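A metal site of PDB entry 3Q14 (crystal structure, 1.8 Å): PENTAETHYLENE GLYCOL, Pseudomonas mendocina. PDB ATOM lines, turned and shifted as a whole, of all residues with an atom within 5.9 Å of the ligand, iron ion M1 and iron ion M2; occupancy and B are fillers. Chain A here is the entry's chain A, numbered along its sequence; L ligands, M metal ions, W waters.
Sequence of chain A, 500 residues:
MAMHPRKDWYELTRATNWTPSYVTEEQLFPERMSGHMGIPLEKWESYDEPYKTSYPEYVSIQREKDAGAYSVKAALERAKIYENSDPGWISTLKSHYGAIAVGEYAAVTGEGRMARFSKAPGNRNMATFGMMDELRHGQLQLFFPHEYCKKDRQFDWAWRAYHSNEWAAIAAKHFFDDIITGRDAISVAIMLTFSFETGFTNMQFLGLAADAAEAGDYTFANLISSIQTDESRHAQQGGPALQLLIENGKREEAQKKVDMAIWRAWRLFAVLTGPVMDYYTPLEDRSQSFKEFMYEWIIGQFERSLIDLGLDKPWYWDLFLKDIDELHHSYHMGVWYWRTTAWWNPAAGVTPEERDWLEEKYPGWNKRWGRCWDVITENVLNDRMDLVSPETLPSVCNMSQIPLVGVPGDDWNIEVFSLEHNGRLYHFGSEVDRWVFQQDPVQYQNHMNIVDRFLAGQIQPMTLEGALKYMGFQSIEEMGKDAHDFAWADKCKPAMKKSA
Ile 100 touches the ligand. Gly 103 touches the ligand. Ala 107 touches the ligand (CB to C4, 3.7 Å). Phe 176 touches the ligand. Phe 196 touches the ligand. Thr 201 touches the ligand (CG2 to C6, 3.99 Å). Hydrophobic or aromatic side chains that line the ligand: Ala 107, Phe 176 and Phe 196. Ten residues have an atom within 4 Å of the ligand: Ile 100, Gly 103, Glu 104, Ala 107, Glu 134, Phe 176, Phe 196, Glu 197, Thr 201 and Glu 231.
The side-chain carboxylate (OE1) of Glu 104 lies close to the side-chain amide oxygen (OE1) of Gln 141. The side-chain hydroxyl (OG1) of Thr 201 lies within hydrogen-bond range of the backbone carbonyl oxygen (O) of Glu 197 (3.3 Å). The backbone NH (N) of Glu 197 sits at hydrogen-bond distance from the backbone carbonyl oxygen (O) of Leu 192 (2.9 Å). OG1 of Thr 201 is in hydrogen-bond range of OE1 of Glu 231 (2.7 Å). A ring nitrogen (NE2) of His 137 lies within hydrogen-bond range of the backbone carbonyl oxygen of Ile 227, 3.5 Å away. NE2 of His 137 lies close to O of Asp 133 (3.4 Å). The backbone carbonyl oxygen of His 137 sits close to the side-chain amide oxygen of Gln 141 (3.2 Å). The side-chain carboxylate (OD2) of Asp 133 sits at hydrogen-bond distance from a ring nitrogen (ND1) of His 234 (2.8 Å).
Iron ion M2 is bound by OE2 of Glu 104 (2.1 Å), water W2 (2.1 Å), OE1 of Glu 134 (2.1 Å), water W1 (2.1 Å) and ND1 of His 137 (2.1 Å). Iron ion M2 has five donor atoms within binding distance.
Iron ion M1 is bound by water W2 (2.0 Å), the side-chain carboxylate (OE2) of Glu 197 (2.1 Å), the side-chain carboxylate (OE2) of Glu 231 (2.1 Å), the side-chain carboxylate (OE2) of Glu 134 (2.1 Å), a ring nitrogen (NE2) of His 234 (2.2 Å) and an oxygen (O1) of the ligand (2.2 Å).
Four residues have an atom within 4 Å of iron ion M1: Glu 134, Glu 197, Glu 231 and His 234.
Within 4 Å of iron ion M2: Glu 104, Glu 134 and His 137. The nearest printed residue that does not touch iron ion M2 is Ile 227 (4.5 Å).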
ATOM      1  N   ALA A  99     -10.328 -20.419  14.500  1.00  0.00           N
ATOM      2  CA  ALA A  99     -11.198 -20.037  15.612  1.00  0.00           C
ATOM      3  C   ALA A  99     -12.580 -19.581  15.150  1.00  0.00           C
ATOM      4  O   ALA A  99     -13.542 -19.638  15.920  1.00  0.00           O
ATOM      5  CB  ALA A  99     -10.535 -18.955  16.447  1.00  0.00           C
ATOM      6  N   ILE A 100     -12.674 -19.142  13.894  1.00  0.00           N
ATOM      7  CA  ILE A 100     -13.835 -18.382  13.432  1.00  0.00           C
ATOM      8  C   ILE A 100     -14.721 -19.090  12.417  1.00  0.00           C
ATOM      9  O   ILE A 100     -15.945 -19.056  12.531  1.00  0.00           O
ATOM     10  CB  ILE A 100     -13.385 -17.025  12.859  1.00  0.00           C
ATOM     11  CG1 ILE A 100     -12.735 -16.176  13.947  1.00  0.00           C
ATOM     12  CG2 ILE A 100     -14.565 -16.290  12.195  1.00  0.00           C
ATOM     13  CD1 ILE A 100     -13.665 -15.797  15.081  1.00  0.00           C
ATOM     14  N   GLY A 103     -17.379 -21.549  13.602  1.00  0.00           N
ATOM     15  CA  GLY A 103     -18.181 -20.805  14.566  1.00  0.00           C
ATOM     16  C   GLY A 103     -19.185 -19.886  13.888  1.00  0.00           C
ATOM     17  O   GLY A 103     -20.322 -19.722  14.367  1.00  0.00           O
ATOM     18  N   GLU A 104     -18.781 -19.249  12.791  1.00  0.00           N
ATOM     19  CA  GLU A 104     -19.717 -18.471  11.973  1.00  0.00           C
ATOM     20  C   GLU A 104     -20.855 -19.369  11.529  1.00  0.00           C
ATOM     21  O   GLU A 104     -22.015 -18.992  11.567  1.00  0.00           O
ATOM     22  CB  GLU A 104     -19.024 -17.907  10.724  1.00  0.00           C
ATOM     23  CG  GLU A 104     -17.901 -16.946  11.040  1.00  0.00           C
ATOM     24  CD  GLU A 104     -18.352 -15.506  11.057  1.00  0.00           C
ATOM     25  OE1 GLU A 104     -17.493 -14.627  10.864  1.00  0.00           O
ATOM     26  OE2 GLU A 104     -19.560 -15.262  11.266  1.00  0.00           O
ATOM     27  N   ALA A 107     -23.255 -19.863  14.142  1.00  0.00           N
ATOM     28  CA  ALA A 107     -24.114 -18.709  14.370  1.00  0.00           C
ATOM     29  C   ALA A 107     -25.363 -18.748  13.494  1.00  0.00           C
ATOM     30  O   ALA A 107     -26.354 -18.085  13.799  1.00  0.00           O
ATOM     31  CB  ALA A 107     -23.343 -17.401  14.136  1.00  0.00           C
ATOM     32  N   GLU A 111     -29.178 -17.618  14.781  1.00  0.00           N
ATOM     33  CA  GLU A 111     -30.119 -16.818  13.999  1.00  0.00           C
ATOM     34  C   GLU A 111     -31.378 -17.631  13.715  1.00  0.00           C
ATOM     35  O   GLU A 111     -32.489 -17.111  13.804  1.00  0.00           O
ATOM     36  CB  GLU A 111     -29.472 -16.307  12.715  1.00  0.00           C
ATOM     37  CG  GLU A 111     -28.355 -15.291  12.943  1.00  0.00           C
ATOM     38  CD  GLU A 111     -28.875 -13.894  13.341  1.00  0.00           C
ATOM     39  OE1 GLU A 111     -30.082 -13.642  13.221  1.00  0.00           O
ATOM     40  OE2 GLU A 111     -28.057 -13.053  13.766  1.00  0.00           O
ATOM     41  N   ASP A 133     -26.534 -14.249   6.359  1.00  0.00           N
ATOM     42  CA  ASP A 133     -25.255 -13.593   6.580  1.00  0.00           C
ATOM     43  C   ASP A 133     -24.228 -14.569   7.184  1.00  0.00           C
ATOM     44  O   ASP A 133     -23.077 -14.578   6.794  1.00  0.00           O
ATOM     45  CB  ASP A 133     -25.375 -12.426   7.566  1.00  0.00           C
ATOM     46  CG  ASP A 133     -26.182 -11.259   7.034  1.00  0.00           C
ATOM     47  OD1 ASP A 133     -26.306 -11.096   5.801  1.00  0.00           O
ATOM     48  OD2 ASP A 133     -26.651 -10.469   7.891  1.00  0.00           O
ATOM     49  N   GLU A 134     -24.627 -15.331   8.189  1.00  0.00           N
ATOM     50  CA  GLU A 134     -23.664 -16.204   8.846  1.00  0.00           C
ATOM     51  C   GLU A 134     -23.267 -17.354   7.921  1.00  0.00           C
ATOM     52  O   GLU A 134     -22.148 -17.848   7.973  1.00  0.00           O
ATOM     53  CB  GLU A 134     -24.171 -16.736  10.194  1.00  0.00           C
ATOM     54  CG  GLU A 134     -24.559 -15.645  11.233  1.00  0.00           C
ATOM     55  CD  GLU A 134     -23.404 -14.704  11.614  1.00  0.00           C
ATOM     56  OE1 GLU A 134     -22.299 -14.762  11.042  1.00  0.00           O
ATOM     57  OE2 GLU A 134     -23.614 -13.919  12.555  1.00  0.00           O
ATOM     58  N   HIS A 137     -20.608 -15.924   5.915  1.00  0.00           N
ATOM     59  CA  HIS A 137     -19.363 -15.782   6.654  1.00  0.00           C
ATOM     60  C   HIS A 137     -18.647 -17.095   6.837  1.00  0.00           C
ATOM     61  O   HIS A 137     -17.438 -17.153   6.714  1.00  0.00           O
ATOM     62  CB  HIS A 137     -19.609 -15.137   8.000  1.00  0.00           C
ATOM     63  CG  HIS A 137     -20.249 -13.790   7.892  1.00  0.00           C
ATOM     64  ND1 HIS A 137     -20.737 -13.112   8.982  1.00  0.00           N
ATOM     65  CD2 HIS A 137     -20.471 -12.996   6.816  1.00  0.00           C
ATOM     66  CE1 HIS A 137     -21.240 -11.955   8.587  1.00  0.00           C
ATOM     67  NE2 HIS A 137     -21.100 -11.863   7.270  1.00  0.00           N
ATOM     68  N   GLN A 141     -15.041 -17.967   4.986  1.00  0.00           N
ATOM     69  CA  GLN A 141     -13.882 -18.215   5.819  1.00  0.00           C
ATOM     70  C   GLN A 141     -13.413 -19.663   5.812  1.00  0.00           C
ATOM     71  O   GLN A 141     -12.425 -20.000   6.436  1.00  0.00           O
ATOM     72  CB  GLN A 141     -14.111 -17.644   7.230  1.00  0.00           C
ATOM     73  CG  GLN A 141     -14.075 -16.114   7.177  1.00  0.00           C
ATOM     74  CD  GLN A 141     -14.542 -15.469   8.455  1.00  0.00           C
ATOM     75  OE1 GLN A 141     -15.698 -15.626   8.852  1.00  0.00           O
ATOM     76  NE2 GLN A 141     -13.650 -14.738   9.093  1.00  0.00           N
ATOM     77  N   TYR A 162     -13.144 -27.025  15.078  1.00  0.00           N
ATOM     78  CA  TYR A 162     -14.360 -27.272  15.842  1.00  0.00           C
ATOM     79  C   TYR A 162     -14.716 -28.744  15.904  1.00  0.00           C
ATOM     80  O   TYR A 162     -15.549 -29.152  16.695  1.00  0.00           O
ATOM     81  CB  TYR A 162     -15.536 -26.458  15.288  1.00  0.00           C
ATOM     82  CG  TYR A 162     -15.545 -24.995  15.701  1.00  0.00           C
ATOM     83  CD1 TYR A 162     -14.518 -24.138  15.348  1.00  0.00           C
ATOM     84  CD2 TYR A 162     -16.596 -24.479  16.448  1.00  0.00           C
ATOM     85  CE1 TYR A 162     -14.530 -22.803  15.724  1.00  0.00           C
ATOM     86  CE2 TYR A 162     -16.625 -23.130  16.836  1.00  0.00           C
ATOM     87  CZ  TYR A 162     -15.587 -22.301  16.461  1.00  0.00           C
ATOM     88  OH  TYR A 162     -15.596 -20.979  16.832  1.00  0.00           O
ATOM     89  N   PHE A 176     -19.342 -20.454  22.388  1.00  0.00           N
ATOM     90  CA  PHE A 176     -20.361 -20.287  21.344  1.00  0.00           C
ATOM     91  C   PHE A 176     -21.575 -21.155  21.627  1.00  0.00           C
ATOM     92  O   PHE A 176     -22.705 -20.758  21.342  1.00  0.00           O
ATOM     93  CB  PHE A 176     -19.771 -20.516  19.955  1.00  0.00           C
ATOM     94  CG  PHE A 176     -18.860 -19.422  19.520  1.00  0.00           C
ATOM     95  CD1 PHE A 176     -19.262 -18.093  19.616  1.00  0.00           C
ATOM     96  CD2 PHE A 176     -17.575 -19.700  19.083  1.00  0.00           C
ATOM     97  CE1 PHE A 176     -18.415 -17.066  19.234  1.00  0.00           C
ATOM     98  CE2 PHE A 176     -16.725 -18.675  18.692  1.00  0.00           C
ATOM     99  CZ  PHE A 176     -17.142 -17.361  18.775  1.00  0.00           C
ATOM    100  N   ILE A 180     -24.663 -18.867  21.649  1.00  0.00           N
ATOM    101  CA  ILE A 180     -25.259 -18.954  20.320  1.00  0.00           C
ATOM    102  C   ILE A 180     -26.252 -20.101  20.175  1.00  0.00           C
ATOM    103  O   ILE A 180     -27.402 -19.893  19.798  1.00  0.00           O
ATOM    104  CB  ILE A 180     -24.198 -19.137  19.207  1.00  0.00           C
ATOM    105  CG1 ILE A 180     -23.206 -17.975  19.234  1.00  0.00           C
ATOM    106  CG2 ILE A 180     -24.880 -19.269  17.835  1.00  0.00           C
ATOM    107  CD1 ILE A 180     -22.321 -17.922  17.972  1.00  0.00           C
ATOM    108  N   LEU A 192     -25.704 -12.916  21.861  1.00  0.00           N
ATOM    109  CA  LEU A 192     -25.021 -12.949  20.591  1.00  0.00           C
ATOM    110  C   LEU A 192     -25.143 -11.609  19.860  1.00  0.00           C
ATOM    111  O   LEU A 192     -24.154 -10.929  19.640  1.00  0.00           O
ATOM    112  CB  LEU A 192     -25.554 -14.078  19.711  1.00  0.00           C
ATOM    113  CG  LEU A 192     -25.025 -14.073  18.265  1.00  0.00           C
ATOM    114  CD1 LEU A 192     -23.515 -14.230  18.228  1.00  0.00           C
ATOM    115  CD2 LEU A 192     -25.709 -15.194  17.502  1.00  0.00           C
ATOM    116  N   PHE A 196     -22.028  -9.838  22.000  1.00  0.00           N
ATOM    117  CA  PHE A 196     -20.893 -10.294  21.211  1.00  0.00           C
ATOM    118  C   PHE A 196     -20.735  -9.490  19.913  1.00  0.00           C
ATOM    119  O   PHE A 196     -19.633  -9.013  19.591  1.00  0.00           O
ATOM    120  CB  PHE A 196     -21.032 -11.790  20.918  1.00  0.00           C
ATOM    121  CG  PHE A 196     -19.851 -12.383  20.192  1.00  0.00           C
ATOM    122  CD1 PHE A 196     -18.608 -12.435  20.791  1.00  0.00           C
ATOM    123  CD2 PHE A 196     -20.012 -12.924  18.930  1.00  0.00           C
ATOM    124  CE1 PHE A 196     -17.525 -12.999  20.119  1.00  0.00           C
ATOM    125  CE2 PHE A 196     -18.920 -13.488  18.261  1.00  0.00           C
ATOM    126  CZ  PHE A 196     -17.690 -13.528  18.862  1.00  0.00           C
ATOM    127  N   GLU A 197     -21.834  -9.326  19.177  1.00  0.00           N
ATOM    128  CA  GLU A 197     -21.734  -8.801  17.802  1.00  0.00           C
ATOM    129  C   GLU A 197     -21.711  -7.276  17.701  1.00  0.00           C
ATOM    130  O   GLU A 197     -21.235  -6.744  16.701  1.00  0.00           O
ATOM    131  CB  GLU A 197     -22.825  -9.367  16.894  1.00  0.00           C
ATOM    132  CG  GLU A 197     -22.752 -10.883  16.704  1.00  0.00           C
ATOM    133  CD  GLU A 197     -23.856 -11.419  15.792  1.00  0.00           C
ATOM    134  OE1 GLU A 197     -25.011 -10.955  15.904  1.00  0.00           O
ATOM    135  OE2 GLU A 197     -23.562 -12.292  14.971  1.00  0.00           O
ATOM    136  N   THR A 201     -16.896  -8.306  18.331  1.00  0.00           N
ATOM    137  CA  THR A 201     -16.382  -8.756  17.041  1.00  0.00           C
ATOM    138  C   THR A 201     -15.640  -7.673  16.282  1.00  0.00           C
ATOM    139  O   THR A 201     -14.762  -7.966  15.470  1.00  0.00           O
ATOM    140  CB  THR A 201     -17.448  -9.364  16.134  1.00  0.00           C
ATOM    141  OG1 THR A 201     -18.505  -8.420  15.946  1.00  0.00           O
ATOM    142  CG2 THR A 201     -18.014 -10.647  16.737  1.00  0.00           C
ATOM    143  N   PHE A 205     -12.569  -8.264  13.612  1.00  0.00           N
ATOM    144  CA  PHE A 205     -12.862  -8.078  12.191  1.00  0.00           C
ATOM    145  C   PHE A 205     -12.511  -6.681  11.643  1.00  0.00           C
ATOM    146  O   PHE A 205     -12.436  -6.496  10.416  1.00  0.00           O
ATOM    147  CB  PHE A 205     -14.328  -8.395  11.906  1.00  0.00           C
ATOM    148  CG  PHE A 205     -14.640  -9.862  12.018  1.00  0.00           C
ATOM    149  CD1 PHE A 205     -14.867 -10.451  13.262  1.00  0.00           C
ATOM    150  CD2 PHE A 205     -14.671 -10.645  10.888  1.00  0.00           C
ATOM    151  CE1 PHE A 205     -15.140 -11.800  13.350  1.00  0.00           C
ATOM    152  CE2 PHE A 205     -14.935 -12.002  10.983  1.00  0.00           C
ATOM    153  CZ  PHE A 205     -15.181 -12.574  12.214  1.00  0.00           C
ATOM    154  N   ILE A 227     -17.150  -8.690   5.784  1.00  0.00           N
ATOM    155  CA  ILE A 227     -17.930  -9.488   6.703  1.00  0.00           C
ATOM    156  C   ILE A 227     -18.584  -8.597   7.768  1.00  0.00           C
ATOM    157  O   ILE A 227     -19.755  -8.757   8.092  1.00  0.00           O
ATOM    158  CB  ILE A 227     -17.065 -10.605   7.322  1.00  0.00           C
ATOM    159  CG1 ILE A 227     -16.879 -11.707   6.284  1.00  0.00           C
ATOM    160  CG2 ILE A 227     -17.702 -11.172   8.596  1.00  0.00           C
ATOM    161  CD1 ILE A 227     -15.807 -12.754   6.670  1.00  0.00           C
ATOM    162  N   GLU A 231     -22.465  -7.894   9.836  1.00  0.00           N
ATOM    163  CA  GLU A 231     -22.567  -7.919  11.293  1.00  0.00           C
ATOM    164  C   GLU A 231     -23.257  -6.647  11.754  1.00  0.00           C
ATOM    165  O   GLU A 231     -24.137  -6.674  12.614  1.00  0.00           O
ATOM    166  CB  GLU A 231     -21.162  -7.991  11.896  1.00  0.00           C
ATOM    167  CG  GLU A 231     -21.138  -8.045  13.425  1.00  0.00           C
ATOM    168  CD  GLU A 231     -21.259  -9.466  13.938  1.00  0.00           C
ATOM    169  OE1 GLU A 231     -20.352  -9.940  14.654  1.00  0.00           O
ATOM    170  OE2 GLU A 231     -22.264 -10.115  13.611  1.00  0.00           O
ATOM    171  N   HIS A 234     -27.145  -7.188  11.162  1.00  0.00           N
ATOM    172  CA  HIS A 234     -27.890  -8.166  11.952  1.00  0.00           C
ATOM    173  C   HIS A 234     -27.660  -8.071  13.458  1.00  0.00           C
ATOM    174  O   HIS A 234     -28.495  -8.515  14.239  1.00  0.00           O
ATOM    175  CB  HIS A 234     -27.746  -9.613  11.430  1.00  0.00           C
ATOM    176  CG  HIS A 234     -26.376 -10.199  11.558  1.00  0.00           C
ATOM    177  ND1 HIS A 234     -25.684 -10.671  10.459  1.00  0.00           N
ATOM    178  CD2 HIS A 234     -25.611 -10.483  12.628  1.00  0.00           C
ATOM    179  CE1 HIS A 234     -24.535 -11.182  10.846  1.00  0.00           C
ATOM    180  NE2 HIS A 234     -24.461 -11.085  12.164  1.00  0.00           N
HETATM  181  C1  LIG L   1     -17.638 -17.144  15.557  1.00  0.00           C
HETATM  182  C2  LIG L   1     -18.477 -15.980  15.114  1.00  0.00           C
HETATM  183  C3  LIG L   1     -19.863 -16.083  15.129  1.00  0.00           C
HETATM  184  C4  LIG L   1     -20.639 -15.013  14.719  1.00  0.00           C
HETATM  185  C5  LIG L   1     -17.865 -14.810  14.714  1.00  0.00           C
HETATM  186  C6  LIG L   1     -18.637 -13.733  14.292  1.00  0.00           C
HETATM  187  C7  LIG L   1     -20.020 -13.839  14.298  1.00  0.00           C
HETATM  188  O1  LIG L   1     -20.787 -12.768  13.892  1.00  0.00           O
HETATM  189 FE    FE M   1     -22.740 -12.062  13.094  1.00  0.00          FE
HETATM  190 FE    FE M   2     -20.593 -13.497  11.075  1.00  0.00          FE
HETATM  191  O   HOH W   1     -18.771 -12.415  11.261  1.00  0.00           O
HETATM  192  O   HOH W   2     -21.574 -11.701  11.493  1.00  0.00           O
HETATM  193  O   HOH W   3     -18.446 -10.478  12.895  1.00  0.00           O
